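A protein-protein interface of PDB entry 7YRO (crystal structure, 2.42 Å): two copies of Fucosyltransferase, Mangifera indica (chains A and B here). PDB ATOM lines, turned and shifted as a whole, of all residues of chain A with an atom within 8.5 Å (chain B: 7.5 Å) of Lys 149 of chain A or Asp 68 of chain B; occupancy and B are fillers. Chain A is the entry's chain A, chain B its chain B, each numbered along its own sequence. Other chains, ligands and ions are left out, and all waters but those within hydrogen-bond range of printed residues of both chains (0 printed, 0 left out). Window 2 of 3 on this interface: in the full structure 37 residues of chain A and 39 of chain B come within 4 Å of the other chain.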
ATOM      1  N   MET A 109      -1.012 -34.505  17.131  1.00  0.00           N
ATOM      2  CA  MET A 109      -0.764 -33.152  16.656  1.00  0.00           C
ATOM      3  C   MET A 109      -1.265 -32.169  17.700  1.00  0.00           C
ATOM      4  O   MET A 109      -2.413 -32.266  18.145  1.00  0.00           O
ATOM      5  CB  MET A 109      -1.465 -32.897  15.318  1.00  0.00           C
ATOM      6  CG  MET A 109      -1.036 -33.829  14.204  1.00  0.00           C
ATOM      7  SD  MET A 109      -2.180 -33.762  12.815  1.00  0.00           S
ATOM      8  CE  MET A 109      -1.471 -32.431  11.845  1.00  0.00           C
ATOM      9  N   HIS A 111      -1.555 -28.971  17.007  1.00  0.00           N
ATOM     10  CA  HIS A 111      -2.322 -28.001  16.236  1.00  0.00           C
ATOM     11  C   HIS A 111      -2.897 -28.672  14.998  1.00  0.00           C
ATOM     12  O   HIS A 111      -2.200 -29.426  14.313  1.00  0.00           O
ATOM     13  CB  HIS A 111      -1.473 -26.801  15.809  1.00  0.00           C
ATOM     14  CG  HIS A 111      -2.193 -25.859  14.897  1.00  0.00           C
ATOM     15  ND1 HIS A 111      -3.104 -24.931  15.355  1.00  0.00           N
ATOM     16  CD2 HIS A 111      -2.147 -25.708  13.552  1.00  0.00           C
ATOM     17  CE1 HIS A 111      -3.586 -24.248  14.333  1.00  0.00           C
ATOM     18  NE2 HIS A 111      -3.020 -24.698  13.227  1.00  0.00           N
ATOM     19  N   VAL A 112      -4.167 -28.385  14.706  1.00  0.00           N
ATOM     20  CA  VAL A 112      -4.851 -28.930  13.538  1.00  0.00           C
ATOM     21  C   VAL A 112      -5.527 -27.789  12.788  1.00  0.00           C
ATOM     22  O   VAL A 112      -6.191 -26.943  13.400  1.00  0.00           O
ATOM     23  CB  VAL A 112      -5.888 -30.003  13.926  1.00  0.00           C
ATOM     24  CG1 VAL A 112      -6.697 -30.423  12.713  1.00  0.00           C
ATOM     25  CG2 VAL A 112      -5.198 -31.203  14.541  1.00  0.00           C
ATOM     26  N   SER A 113      -5.377 -27.778  11.467  1.00  0.00           N
ATOM     27  CA  SER A 113      -6.034 -26.799  10.615  1.00  0.00           C
ATOM     28  C   SER A 113      -7.055 -27.488   9.719  1.00  0.00           C
ATOM     29  O   SER A 113      -6.785 -28.553   9.154  1.00  0.00           O
ATOM     30  CB  SER A 113      -5.012 -26.026   9.777  1.00  0.00           C
ATOM     31  OG  SER A 113      -4.287 -26.873   8.902  1.00  0.00           O
ATOM     32  N   VAL A 114      -8.234 -26.880   9.617  1.00  0.00           N
ATOM     33  CA  VAL A 114      -9.338 -27.366   8.799  1.00  0.00           C
ATOM     34  C   VAL A 114      -9.760 -26.260   7.840  1.00  0.00           C
ATOM     35  O   VAL A 114     -10.134 -25.156   8.269  1.00  0.00           O
ATOM     36  CB  VAL A 114     -10.527 -27.817   9.661  1.00  0.00           C
ATOM     37  CG1 VAL A 114     -11.721 -28.152   8.779  1.00  0.00           C
ATOM     38  CG2 VAL A 114     -10.132 -29.010  10.506  1.00  0.00           C
ATOM     39  N   LEU A 115      -9.687 -26.559   6.545  1.00  0.00           N
ATOM     40  CA  LEU A 115     -10.179 -25.686   5.491  1.00  0.00           C
ATOM     41  C   LEU A 115     -11.519 -26.223   4.998  1.00  0.00           C
ATOM     42  O   LEU A 115     -11.601 -27.363   4.532  1.00  0.00           O
ATOM     43  CB  LEU A 115      -9.171 -25.607   4.346  1.00  0.00           C
ATOM     44  CG  LEU A 115      -9.599 -24.856   3.084  1.00  0.00           C
ATOM     45  CD1 LEU A 115      -9.892 -23.398   3.400  1.00  0.00           C
ATOM     46  CD2 LEU A 115      -8.527 -24.967   2.010  1.00  0.00           C
ATOM     47  N   SER A 143     -10.984 -19.728   4.313  1.00  0.00           N
ATOM     48  CA  SER A 143     -10.013 -18.959   3.547  1.00  0.00           C
ATOM     49  C   SER A 143      -8.760 -19.801   3.349  1.00  0.00           C
ATOM     50  O   SER A 143      -8.132 -20.230   4.324  1.00  0.00           O
ATOM     51  CB  SER A 143      -9.669 -17.645   4.247  1.00  0.00           C
ATOM     52  OG  SER A 143      -8.556 -17.027   3.624  1.00  0.00           O
ATOM     53  N   SER A 144      -8.399 -20.029   2.087  1.00  0.00           N
ATOM     54  CA  SER A 144      -7.158 -20.718   1.774  1.00  0.00           C
ATOM     55  C   SER A 144      -5.933 -19.845   2.011  1.00  0.00           C
ATOM     56  O   SER A 144      -4.811 -20.351   1.930  1.00  0.00           O
ATOM     57  CB  SER A 144      -7.191 -21.211   0.329  1.00  0.00           C
ATOM     58  OG  SER A 144      -7.631 -20.186  -0.541  1.00  0.00           O
ATOM     59  N   VAL A 145      -6.120 -18.555   2.296  1.00  0.00           N
ATOM     60  CA  VAL A 145      -4.994 -17.716   2.691  1.00  0.00           C
ATOM     61  C   VAL A 145      -4.656 -17.928   4.164  1.00  0.00           C
ATOM     62  O   VAL A 145      -3.478 -18.014   4.533  1.00  0.00           O
ATOM     63  CB  VAL A 145      -5.296 -16.239   2.384  1.00  0.00           C
ATOM     64  CG1 VAL A 145      -4.099 -15.367   2.751  1.00  0.00           C
ATOM     65  CG2 VAL A 145      -5.664 -16.066   0.922  1.00  0.00           C
ATOM     66  N   LEU A 146      -5.675 -18.012   5.027  1.00  0.00           N
ATOM     67  CA  LEU A 146      -5.428 -18.322   6.433  1.00  0.00           C
ATOM     68  C   LEU A 146      -4.808 -19.703   6.591  1.00  0.00           C
ATOM     69  O   LEU A 146      -3.890 -19.893   7.399  1.00  0.00           O
ATOM     70  CB  LEU A 146      -6.731 -18.231   7.230  1.00  0.00           C
ATOM     71  CG  LEU A 146      -7.043 -16.926   7.964  1.00  0.00           C
ATOM     72  CD1 LEU A 146      -8.468 -16.941   8.481  1.00  0.00           C
ATOM     73  CD2 LEU A 146      -6.069 -16.720   9.114  1.00  0.00           C
ATOM     74  N   VAL A 147      -5.297 -20.681   5.830  1.00  0.00           N
ATOM     75  CA  VAL A 147      -4.725 -22.024   5.778  1.00  0.00           C
ATOM     76  C   VAL A 147      -4.499 -22.387   4.320  1.00  0.00           C
ATOM     77  O   VAL A 147      -5.452 -22.709   3.599  1.00  0.00           O
ATOM     78  CB  VAL A 147      -5.602 -23.078   6.464  1.00  0.00           C
ATOM     79  CG1 VAL A 147      -4.745 -24.245   6.860  1.00  0.00           C
ATOM     80  CG2 VAL A 147      -6.232 -22.508   7.710  1.00  0.00           C
ATOM     81  N   ASP A 148      -3.237 -22.362   3.894  1.00  0.00           N
ATOM     82  CA  ASP A 148      -2.868 -22.756   2.544  1.00  0.00           C
ATOM     83  C   ASP A 148      -2.424 -24.208   2.446  1.00  0.00           C
ATOM     84  O   ASP A 148      -2.381 -24.753   1.339  1.00  0.00           O
ATOM     85  CB  ASP A 148      -1.755 -21.844   2.017  1.00  0.00           C
ATOM     86  CG  ASP A 148      -0.495 -21.911   2.863  1.00  0.00           C
ATOM     87  OD1 ASP A 148      -0.558 -21.563   4.063  1.00  0.00           O
ATOM     88  OD2 ASP A 148       0.561 -22.315   2.330  1.00  0.00           O
ATOM     89  N   LYS A 149      -2.103 -24.846   3.569  1.00  0.00           N
ATOM     90  CA  LYS A 149      -1.762 -26.267   3.608  1.00  0.00           C
ATOM     91  C   LYS A 149      -2.559 -26.927   4.724  1.00  0.00           C
ATOM     92  O   LYS A 149      -2.006 -27.305   5.764  1.00  0.00           O
ATOM     93  CB  LYS A 149      -0.261 -26.478   3.804  1.00  0.00           C
ATOM     94  CG  LYS A 149       0.571 -26.154   2.582  1.00  0.00           C
ATOM     95  CD  LYS A 149       2.030 -26.500   2.818  1.00  0.00           C
ATOM     96  CE  LYS A 149       2.608 -25.702   3.977  1.00  0.00           C
ATOM     97  NZ  LYS A 149       4.042 -26.029   4.228  1.00  0.00           N
ATOM     98  N   PRO A 150      -3.866 -27.086   4.535  1.00  0.00           N
ATOM     99  CA  PRO A 150      -4.707 -27.621   5.610  1.00  0.00           C
ATOM    100  C   PRO A 150      -4.389 -29.077   5.902  1.00  0.00           C
ATOM    101  O   PRO A 150      -3.967 -29.836   5.027  1.00  0.00           O
ATOM    102  CB  PRO A 150      -6.129 -27.459   5.062  1.00  0.00           C
ATOM    103  CG  PRO A 150      -5.956 -27.484   3.584  1.00  0.00           C
ATOM    104  CD  PRO A 150      -4.638 -26.818   3.310  1.00  0.00           C
ATOM    105  N   ASP A 151      -4.582 -29.459   7.163  1.00  0.00           N
ATOM    106  CA  ASP A 151      -4.486 -30.863   7.537  1.00  0.00           C
ATOM    107  C   ASP A 151      -5.707 -31.663   7.112  1.00  0.00           C
ATOM    108  O   ASP A 151      -5.603 -32.884   6.945  1.00  0.00           O
ATOM    109  CB  ASP A 151      -4.305 -30.993   9.048  1.00  0.00           C
ATOM    110  CG  ASP A 151      -3.066 -30.296   9.543  1.00  0.00           C
ATOM    111  OD1 ASP A 151      -2.011 -30.433   8.887  1.00  0.00           O
ATOM    112  OD2 ASP A 151      -3.150 -29.602  10.578  1.00  0.00           O
ATOM    113  N   ALA A 152      -6.854 -31.011   6.933  1.00  0.00           N
ATOM    114  CA  ALA A 152      -8.080 -31.697   6.559  1.00  0.00           C
ATOM    115  C   ALA A 152      -8.977 -30.749   5.778  1.00  0.00           C
ATOM    116  O   ALA A 152      -9.008 -29.548   6.056  1.00  0.00           O
ATOM    117  CB  ALA A 152      -8.819 -32.231   7.791  1.00  0.00           C
ATOM    118  N   LEU A 153      -9.686 -31.289   4.792  1.00  0.00           N
ATOM    119  CA  LEU A 153     -10.693 -30.552   4.039  1.00  0.00           C
ATOM    120  C   LEU A 153     -12.079 -31.050   4.415  1.00  0.00           C
ATOM    121  O   LEU A 153     -12.329 -32.258   4.419  1.00  0.00           O
ATOM    122  CB  LEU A 153     -10.510 -30.679   2.522  1.00  0.00           C
ATOM    123  CG  LEU A 153      -9.391 -30.002   1.729  1.00  0.00           C
ATOM    124  CD1 LEU A 153      -8.065 -30.076   2.419  1.00  0.00           C
ATOM    125  CD2 LEU A 153      -9.309 -30.616   0.340  1.00  0.00           C
ATOM    126  N   GLY A 167      -0.100 -38.289   2.780  1.00  0.00           N
ATOM    127  CA  GLY A 167       0.451 -36.953   2.717  1.00  0.00           C
ATOM    128  C   GLY A 167      -0.489 -35.919   2.138  1.00  0.00           C
ATOM    129  O   GLY A 167      -0.185 -34.719   2.203  1.00  0.00           O
ATOM    130  N   PRO A 169      -4.171 -33.986   2.579  1.00  0.00           N
ATOM    131  CA  PRO A 169      -5.039 -33.713   3.727  1.00  0.00           C
ATOM    132  C   PRO A 169      -6.187 -34.710   3.803  1.00  0.00           C
ATOM    133  O   PRO A 169      -6.673 -35.215   2.789  1.00  0.00           O
ATOM    134  CB  PRO A 169      -5.537 -32.288   3.468  1.00  0.00           C
ATOM    135  CG  PRO A 169      -5.284 -32.042   2.009  1.00  0.00           C
ATOM    136  CD  PRO A 169      -4.083 -32.842   1.656  1.00  0.00           C
ATOM    137  N   ARG A 405      -2.170 -35.443   8.024  1.00  0.00           N
ATOM    138  CA  ARG A 405      -1.704 -35.819   6.694  1.00  0.00           C
ATOM    139  C   ARG A 405      -1.022 -37.182   6.668  1.00  0.00           C
ATOM    140  O   ARG A 405      -0.948 -37.795   5.597  1.00  0.00           O
ATOM    141  CB  ARG A 405      -0.773 -34.748   6.135  1.00  0.00           C
ATOM    142  CG  ARG A 405      -1.547 -33.574   5.588  1.00  0.00           C
ATOM    143  CD  ARG A 405      -0.688 -32.652   4.754  1.00  0.00           C
ATOM    144  NE  ARG A 405      -1.478 -31.532   4.259  1.00  0.00           N
ATOM    145  CZ  ARG A 405      -1.116 -30.728   3.268  1.00  0.00           C
ATOM    146  NH1 ARG A 405       0.023 -30.901   2.616  1.00  0.00           N
ATOM    147  NH2 ARG A 405      -1.907 -29.710   2.937  1.00  0.00           N
ATOM    148  N   ILE B  61       0.825 -16.085  -1.008  1.00  0.00           N
ATOM    149  CA  ILE B  61       1.001 -17.535  -1.055  1.00  0.00           C
ATOM    150  C   ILE B  61       2.332 -17.908  -1.700  1.00  0.00           C
ATOM    151  O   ILE B  61       2.970 -18.893  -1.307  1.00  0.00           O
ATOM    152  CB  ILE B  61      -0.199 -18.199  -1.754  1.00  0.00           C
ATOM    153  CG1 ILE B  61      -1.472 -17.917  -0.949  1.00  0.00           C
ATOM    154  CG2 ILE B  61       0.027 -19.694  -1.909  1.00  0.00           C
ATOM    155  CD1 ILE B  61      -2.745 -18.387  -1.604  1.00  0.00           C
ATOM    156  N   SER B  62       2.763 -17.153  -2.712  1.00  0.00           N
ATOM    157  CA  SER B  62       4.087 -17.394  -3.276  1.00  0.00           C
ATOM    158  C   SER B  62       5.168 -17.202  -2.223  1.00  0.00           C
ATOM    159  O   SER B  62       6.124 -17.984  -2.152  1.00  0.00           O
ATOM    160  CB  SER B  62       4.334 -16.469  -4.464  1.00  0.00           C
ATOM    161  OG  SER B  62       5.654 -16.620  -4.952  1.00  0.00           O
ATOM    162  N   ALA B  63       5.028 -16.163  -1.395  1.00  0.00           N
ATOM    163  CA  ALA B  63       5.957 -15.954  -0.291  1.00  0.00           C
ATOM    164  C   ALA B  63       5.902 -17.112   0.698  1.00  0.00           C
ATOM    165  O   ALA B  63       6.943 -17.566   1.190  1.00  0.00           O
ATOM    166  CB  ALA B  63       5.650 -14.626   0.405  1.00  0.00           C
ATOM    167  N   PHE B  64       4.697 -17.607   0.997  1.00  0.00           N
ATOM    168  CA  PHE B  64       4.570 -18.763   1.882  1.00  0.00           C
ATOM    169  C   PHE B  64       5.303 -19.976   1.327  1.00  0.00           C
ATOM    170  O   PHE B  64       6.012 -20.672   2.063  1.00  0.00           O
ATOM    171  CB  PHE B  64       3.096 -19.105   2.108  1.00  0.00           C
ATOM    172  CG  PHE B  64       2.357 -18.106   2.941  1.00  0.00           C
ATOM    173  CD1 PHE B  64       3.038 -17.186   3.715  1.00  0.00           C
ATOM    174  CD2 PHE B  64       0.971 -18.115   2.973  1.00  0.00           C
ATOM    175  CE1 PHE B  64       2.357 -16.278   4.493  1.00  0.00           C
ATOM    176  CE2 PHE B  64       0.282 -17.209   3.749  1.00  0.00           C
ATOM    177  CZ  PHE B  64       0.974 -16.289   4.511  1.00  0.00           C
ATOM    178  N   LYS B  65       5.125 -20.257   0.037  1.00  0.00           N
ATOM    179  CA  LYS B  65       5.783 -21.408  -0.573  1.00  0.00           C
ATOM    180  C   LYS B  65       7.298 -21.229  -0.618  1.00  0.00           C
ATOM    181  O   LYS B  65       8.048 -22.192  -0.397  1.00  0.00           O
ATOM    182  CB  LYS B  65       5.200 -21.682  -1.959  1.00  0.00           C
ATOM    183  CG  LYS B  65       3.878 -22.460  -1.909  1.00  0.00           C
ATOM    184  CD  LYS B  65       3.963 -23.705  -1.010  1.00  0.00           C
ATOM    185  CE  LYS B  65       2.644 -24.482  -1.058  1.00  0.00           C
ATOM    186  NZ  LYS B  65       2.639 -25.753  -0.283  1.00  0.00           N
ATOM    187  N   LYS B  66       7.770 -20.020  -0.940  1.00  0.00           N
ATOM    188  CA  LYS B  66       9.210 -19.764  -0.921  1.00  0.00           C
ATOM    189  C   LYS B  66       9.789 -19.969   0.476  1.00  0.00           C
ATOM    190  O   LYS B  66      10.880 -20.533   0.628  1.00  0.00           O
ATOM    191  CB  LYS B  66       9.509 -18.350  -1.431  1.00  0.00           C
ATOM    192  CG  LYS B  66       9.999 -18.322  -2.873  1.00  0.00           C
ATOM    193  CD  LYS B  66      10.423 -16.930  -3.323  1.00  0.00           C
ATOM    194  CE  LYS B  66       9.218 -16.020  -3.528  1.00  0.00           C
ATOM    195  NZ  LYS B  66       9.595 -14.747  -4.216  1.00  0.00           N
ATOM    196  N   TRP B  67       9.075 -19.509   1.508  1.00  0.00           N
ATOM    197  CA  TRP B  67       9.510 -19.752   2.880  1.00  0.00           C
ATOM    198  C   TRP B  67       9.500 -21.238   3.212  1.00  0.00           C
ATOM    199  O   TRP B  67      10.380 -21.727   3.930  1.00  0.00           O
ATOM    200  CB  TRP B  67       8.624 -18.990   3.859  1.00  0.00           C
ATOM    201  CG  TRP B  67       9.047 -19.168   5.275  1.00  0.00           C
ATOM    202  CD1 TRP B  67       9.895 -18.371   5.983  1.00  0.00           C
ATOM    203  CD2 TRP B  67       8.646 -20.217   6.162  1.00  0.00           C
ATOM    204  NE1 TRP B  67      10.050 -18.858   7.257  1.00  0.00           N
ATOM    205  CE2 TRP B  67       9.292 -19.993   7.392  1.00  0.00           C
ATOM    206  CE3 TRP B  67       7.803 -21.328   6.035  1.00  0.00           C
ATOM    207  CZ2 TRP B  67       9.123 -20.835   8.486  1.00  0.00           C
ATOM    208  CZ3 TRP B  67       7.639 -22.163   7.123  1.00  0.00           C
ATOM    209  CH2 TRP B  67       8.293 -21.911   8.332  1.00  0.00           C
ATOM    210  N   ASP B  68       8.491 -21.962   2.726  1.00  0.00           N
ATOM    211  CA  ASP B  68       8.415 -23.398   2.977  1.00  0.00           C
ATOM    212  C   ASP B  68       9.615 -24.125   2.388  1.00  0.00           C
ATOM    213  O   ASP B  68      10.197 -25.007   3.032  1.00  0.00           O
ATOM    214  CB  ASP B  68       7.121 -23.958   2.388  1.00  0.00           C
ATOM    215  CG  ASP B  68       5.922 -23.731   3.285  1.00  0.00           C
ATOM    216  OD1 ASP B  68       6.092 -23.707   4.523  1.00  0.00           O
ATOM    217  OD2 ASP B  68       4.804 -23.589   2.751  1.00  0.00           O
ATOM    218  N   SER B  69       9.997 -23.766   1.160  1.00  0.00           N
ATOM    219  CA  SER B  69      11.129 -24.422   0.510  1.00  0.00           C
ATOM    220  C   SER B  69      12.454 -24.013   1.142  1.00  0.00           C
ATOM    221  O   SER B  69      13.350 -24.849   1.316  1.00  0.00           O
ATOM    222  CB  SER B  69      11.122 -24.122  -0.989  1.00  0.00           C
ATOM    223  OG  SER B  69      11.598 -22.815  -1.251  1.00  0.00           O
ATOM    224  N   GLN B  70      12.607 -22.731   1.479  1.00  0.00           N
ATOM    225  CA  GLN B  70      13.891 -22.221   1.941  1.00  0.00           C
ATOM    226  C   GLN B  70      14.084 -22.370   3.446  1.00  0.00           C
ATOM    227  O   GLN B  70      15.214 -22.598   3.892  1.00  0.00           O
ATOM    228  CB  GLN B  70      14.054 -20.749   1.549  1.00  0.00           C
ATOM    229  CG  GLN B  70      14.053 -20.495   0.044  1.00  0.00           C
ATOM    230  CD  GLN B  70      14.480 -19.080  -0.316  1.00  0.00           C
ATOM    231  OE1 GLN B  70      14.677 -18.235   0.558  1.00  0.00           O
ATOM    232  NE2 GLN B  70      14.620 -18.817  -1.612  1.00  0.00           N
ATOM    233  N   VAL B  71      13.021 -22.240   4.242  1.00  0.00           N
ATOM    234  CA  VAL B  71      13.117 -22.282   5.700  1.00  0.00           C
ATOM    235  C   VAL B  71      12.472 -23.550   6.267  1.00  0.00           C
ATOM    236  O   VAL B  71      13.151 -24.386   6.863  1.00  0.00           O
ATOM    237  CB  VAL B  71      12.510 -21.009   6.332  1.00  0.00           C
ATOM    238  CG1 VAL B  71      12.720 -21.011   7.834  1.00  0.00           C
ATOM    239  CG2 VAL B  71      13.122 -19.765   5.704  1.00  0.00           C
ATOM    240  N   GLY B  72      11.170 -23.710   6.088  1.00  0.00           N
ATOM    241  CA  GLY B  72      10.555 -24.949   6.551  1.00  0.00           C
ATOM    242  C   GLY B  72      10.143 -24.901   8.010  1.00  0.00           C
ATOM    243  O   GLY B  72      10.744 -24.220   8.841  1.00  0.00           O
ATOM    244  N   CYS B  73       9.085 -25.656   8.324  1.00  0.00           N
ATOM    245  CA  CYS B  73       8.522 -25.648   9.673  1.00  0.00           C
ATOM    246  C   CYS B  73       9.422 -26.331  10.699  1.00  0.00           C
ATOM    247  O   CYS B  73       9.377 -25.978  11.884  1.00  0.00           O
ATOM    248  CB  CYS B  73       7.146 -26.316   9.670  1.00  0.00           C
ATOM    249  SG  CYS B  73       5.820 -25.311   8.961  1.00  0.00           S
ATOM    250  N   ARG B  75      12.773 -26.250  10.933  1.00  0.00           N
ATOM    251  CA  ARG B  75      13.744 -25.269  11.406  1.00  0.00           C
ATOM    252  C   ARG B  75      13.081 -24.247  12.317  1.00  0.00           C
ATOM    253  O   ARG B  75      13.675 -23.813  13.314  1.00  0.00           O
ATOM    254  CB  ARG B  75      14.425 -24.586  10.219  1.00  0.00           C
ATOM    255  CG  ARG B  75      14.930 -25.559   9.165  1.00  0.00           C
ATOM    256  CD  ARG B  75      16.091 -24.972   8.377  1.00  0.00           C
ATOM    257  NE  ARG B  75      16.339 -25.705   7.141  1.00  0.00           N
ATOM    258  CZ  ARG B  75      16.306 -25.167   5.928  1.00  0.00           C
ATOM    259  NH1 ARG B  75      16.078 -23.875   5.751  1.00  0.00           N
ATOM    260  NH2 ARG B  75      16.518 -25.942   4.868  1.00  0.00           N
ATOM    261  N   VAL B 363      10.479 -14.015   2.032  1.00  0.00           N
ATOM    262  CA  VAL B 363      10.787 -15.120   2.941  1.00  0.00           C
ATOM    263  C   VAL B 363      10.770 -14.648   4.392  1.00  0.00           C
ATOM    264  O   VAL B 363      10.149 -15.272   5.269  1.00  0.00           O
ATOM    265  CB  VAL B 363      12.142 -15.746   2.569  1.00  0.00           C
ATOM    266  CG1 VAL B 363      12.504 -16.852   3.543  1.00  0.00           C
ATOM    267  CG2 VAL B 363      12.109 -16.271   1.145  1.00  0.00           C
ATOM    268  N   ALA B 366       7.235 -14.039   5.458  1.00  0.00           N
ATOM    269  CA  ALA B 366       6.474 -15.250   5.745  1.00  0.00           C
ATOM    270  C   ALA B 366       6.914 -15.926   7.040  1.00  0.00           C
ATOM    271  O   ALA B 366       6.131 -16.686   7.636  1.00  0.00           O
ATOM    272  CB  ALA B 366       6.591 -16.221   4.573  1.00  0.00           C
ATOM    273  N   ALA B 370       4.759 -17.992   9.994  1.00  0.00           N
ATOM    274  CA  ALA B 370       5.116 -19.367  10.331  1.00  0.00           C
ATOM    275  C   ALA B 370       4.434 -19.852  11.610  1.00  0.00           C
ATOM    276  O   ALA B 370       4.218 -21.059  11.771  1.00  0.00           O
ATOM    277  CB  ALA B 370       6.633 -19.492  10.469  1.00  0.00           C
ATOM    278  N   ARG B 373       1.130 -21.056  10.161  1.00  0.00           N
ATOM    279  CA  ARG B 373       1.256 -22.097   9.150  1.00  0.00           C
ATOM    280  C   ARG B 373       1.867 -23.373   9.716  1.00  0.00           C
ATOM    281  O   ARG B 373       1.560 -24.469   9.234  1.00  0.00           O
ATOM    282  CB  ARG B 373       2.063 -21.561   7.970  1.00  0.00           C
ATOM    283  CG  ARG B 373       1.380 -20.367   7.313  1.00  0.00           C
ATOM    284  CD  ARG B 373       2.142 -19.851   6.113  1.00  0.00           C
ATOM    285  NE  ARG B 373       2.016 -20.758   4.983  1.00  0.00           N
ATOM    286  CZ  ARG B 373       2.957 -21.615   4.612  1.00  0.00           C
ATOM    287  NH1 ARG B 373       4.103 -21.706   5.265  1.00  0.00           N
ATOM    288  NH2 ARG B 373       2.736 -22.409   3.569  1.00  0.00           N
ATOM    289  N   CYS B 374       2.719 -23.263  10.734  1.00  0.00           N
ATOM    290  CA  CYS B 374       3.337 -24.429  11.352  1.00  0.00           C
ATOM    291  C   CYS B 374       2.666 -24.837  12.658  1.00  0.00           C
ATOM    292  O   CYS B 374       3.124 -25.785  13.301  1.00  0.00           O
ATOM    293  CB  CYS B 374       4.827 -24.176  11.598  1.00  0.00           C
ATOM    294  SG  CYS B 374       5.748 -23.647  10.132  1.00  0.00           S
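The backbone NH (N) of Val 145 of chain A lies close to the side-chain hydroxyl (OG) of Ser 143 of chain A (3.2 Å).
The side-chain sulfur (SG) of Cys 73 of chain B forms a disulfide with the side-chain sulfur (SG) of Cys 374 of chain B.
OD2 of Asp 68 of chain B lies within salt-bridge range of NH2 of Arg 373 of chain B (2.5 Å).
Of the printed residues of chain B, Val 145 of chain A touches Phe 64.
Lys 149 of chain A touches just these residues of chain B: Lys 65, Asp 68 and Arg 373.
Of the printed residues of chain A, Phe 64 of chain B touches Val 145 (3.9 Å) and Asp 148 (3.9 Å).
Asp 68 of chain B touches just one residue of chain A: Lys 149.
No residue of chain A comes within 4 Å of Ser 69 of chain B.
Of the printed residues of chain A, Arg 373 of chain B touches Asp 148 (2.5 Å) and Lys 149 (3.3 Å).
The nearest residue of chain B that does not touch Lys 149 of chain A is Cys 73 of chain B (5.1 Å).
The nearest residue of chain A that does not touch Asp 68 of chain B is Asp 148 of chain A (4.5 Å).
The nearest printed residue of chain B that does not touch Val 145 of chain A is Ile 61 of chain B (4.5 Å).
No position is printed for both chains.
Of the 6 pairs that touch across the chains among the printed residues, none has its exchanged pair printed and touching as well.
Hydrophobic or aromatic side chains of chain B within 4 Å of the printed part of chain A: Phe 64.
Along chain B the printed residues that touch a printed residue of chain A span positions 64 to 373.
Of the 20 printed residues of chain A, 3 touch a printed residue of chain B.
Among the printed residues, 6 pairs touch across the chains.
Among the printed residues, Asp or Glu carboxylates within 4 Å of a Lys or Arg side-chain nitrogen of the other chain: Asp 148 of chain A with Arg 373 of chain B (2.5 Å) and Lys 149 of chain A with Asp 68 of chain B (3.0 Å).
NZ of Lys 149 of chain A is in salt-bridge range of OD2 of Asp 68 of chain B.
The guanidinium group (NH2) of Arg 373 of chain B is in salt-bridge range of the side-chain carboxylate (OD2) of Asp 148 of chain A (2.5 Å).
Among the printed residues, merely in contact across the chains: Lys 149 of chain A with Lys 65 of chain B, Lys 149 of chain A with Arg 373 of chain B, Val 145 of chain A with Phe 64 of chain B and Asp 148 of chain A with Phe 64 of chain B.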
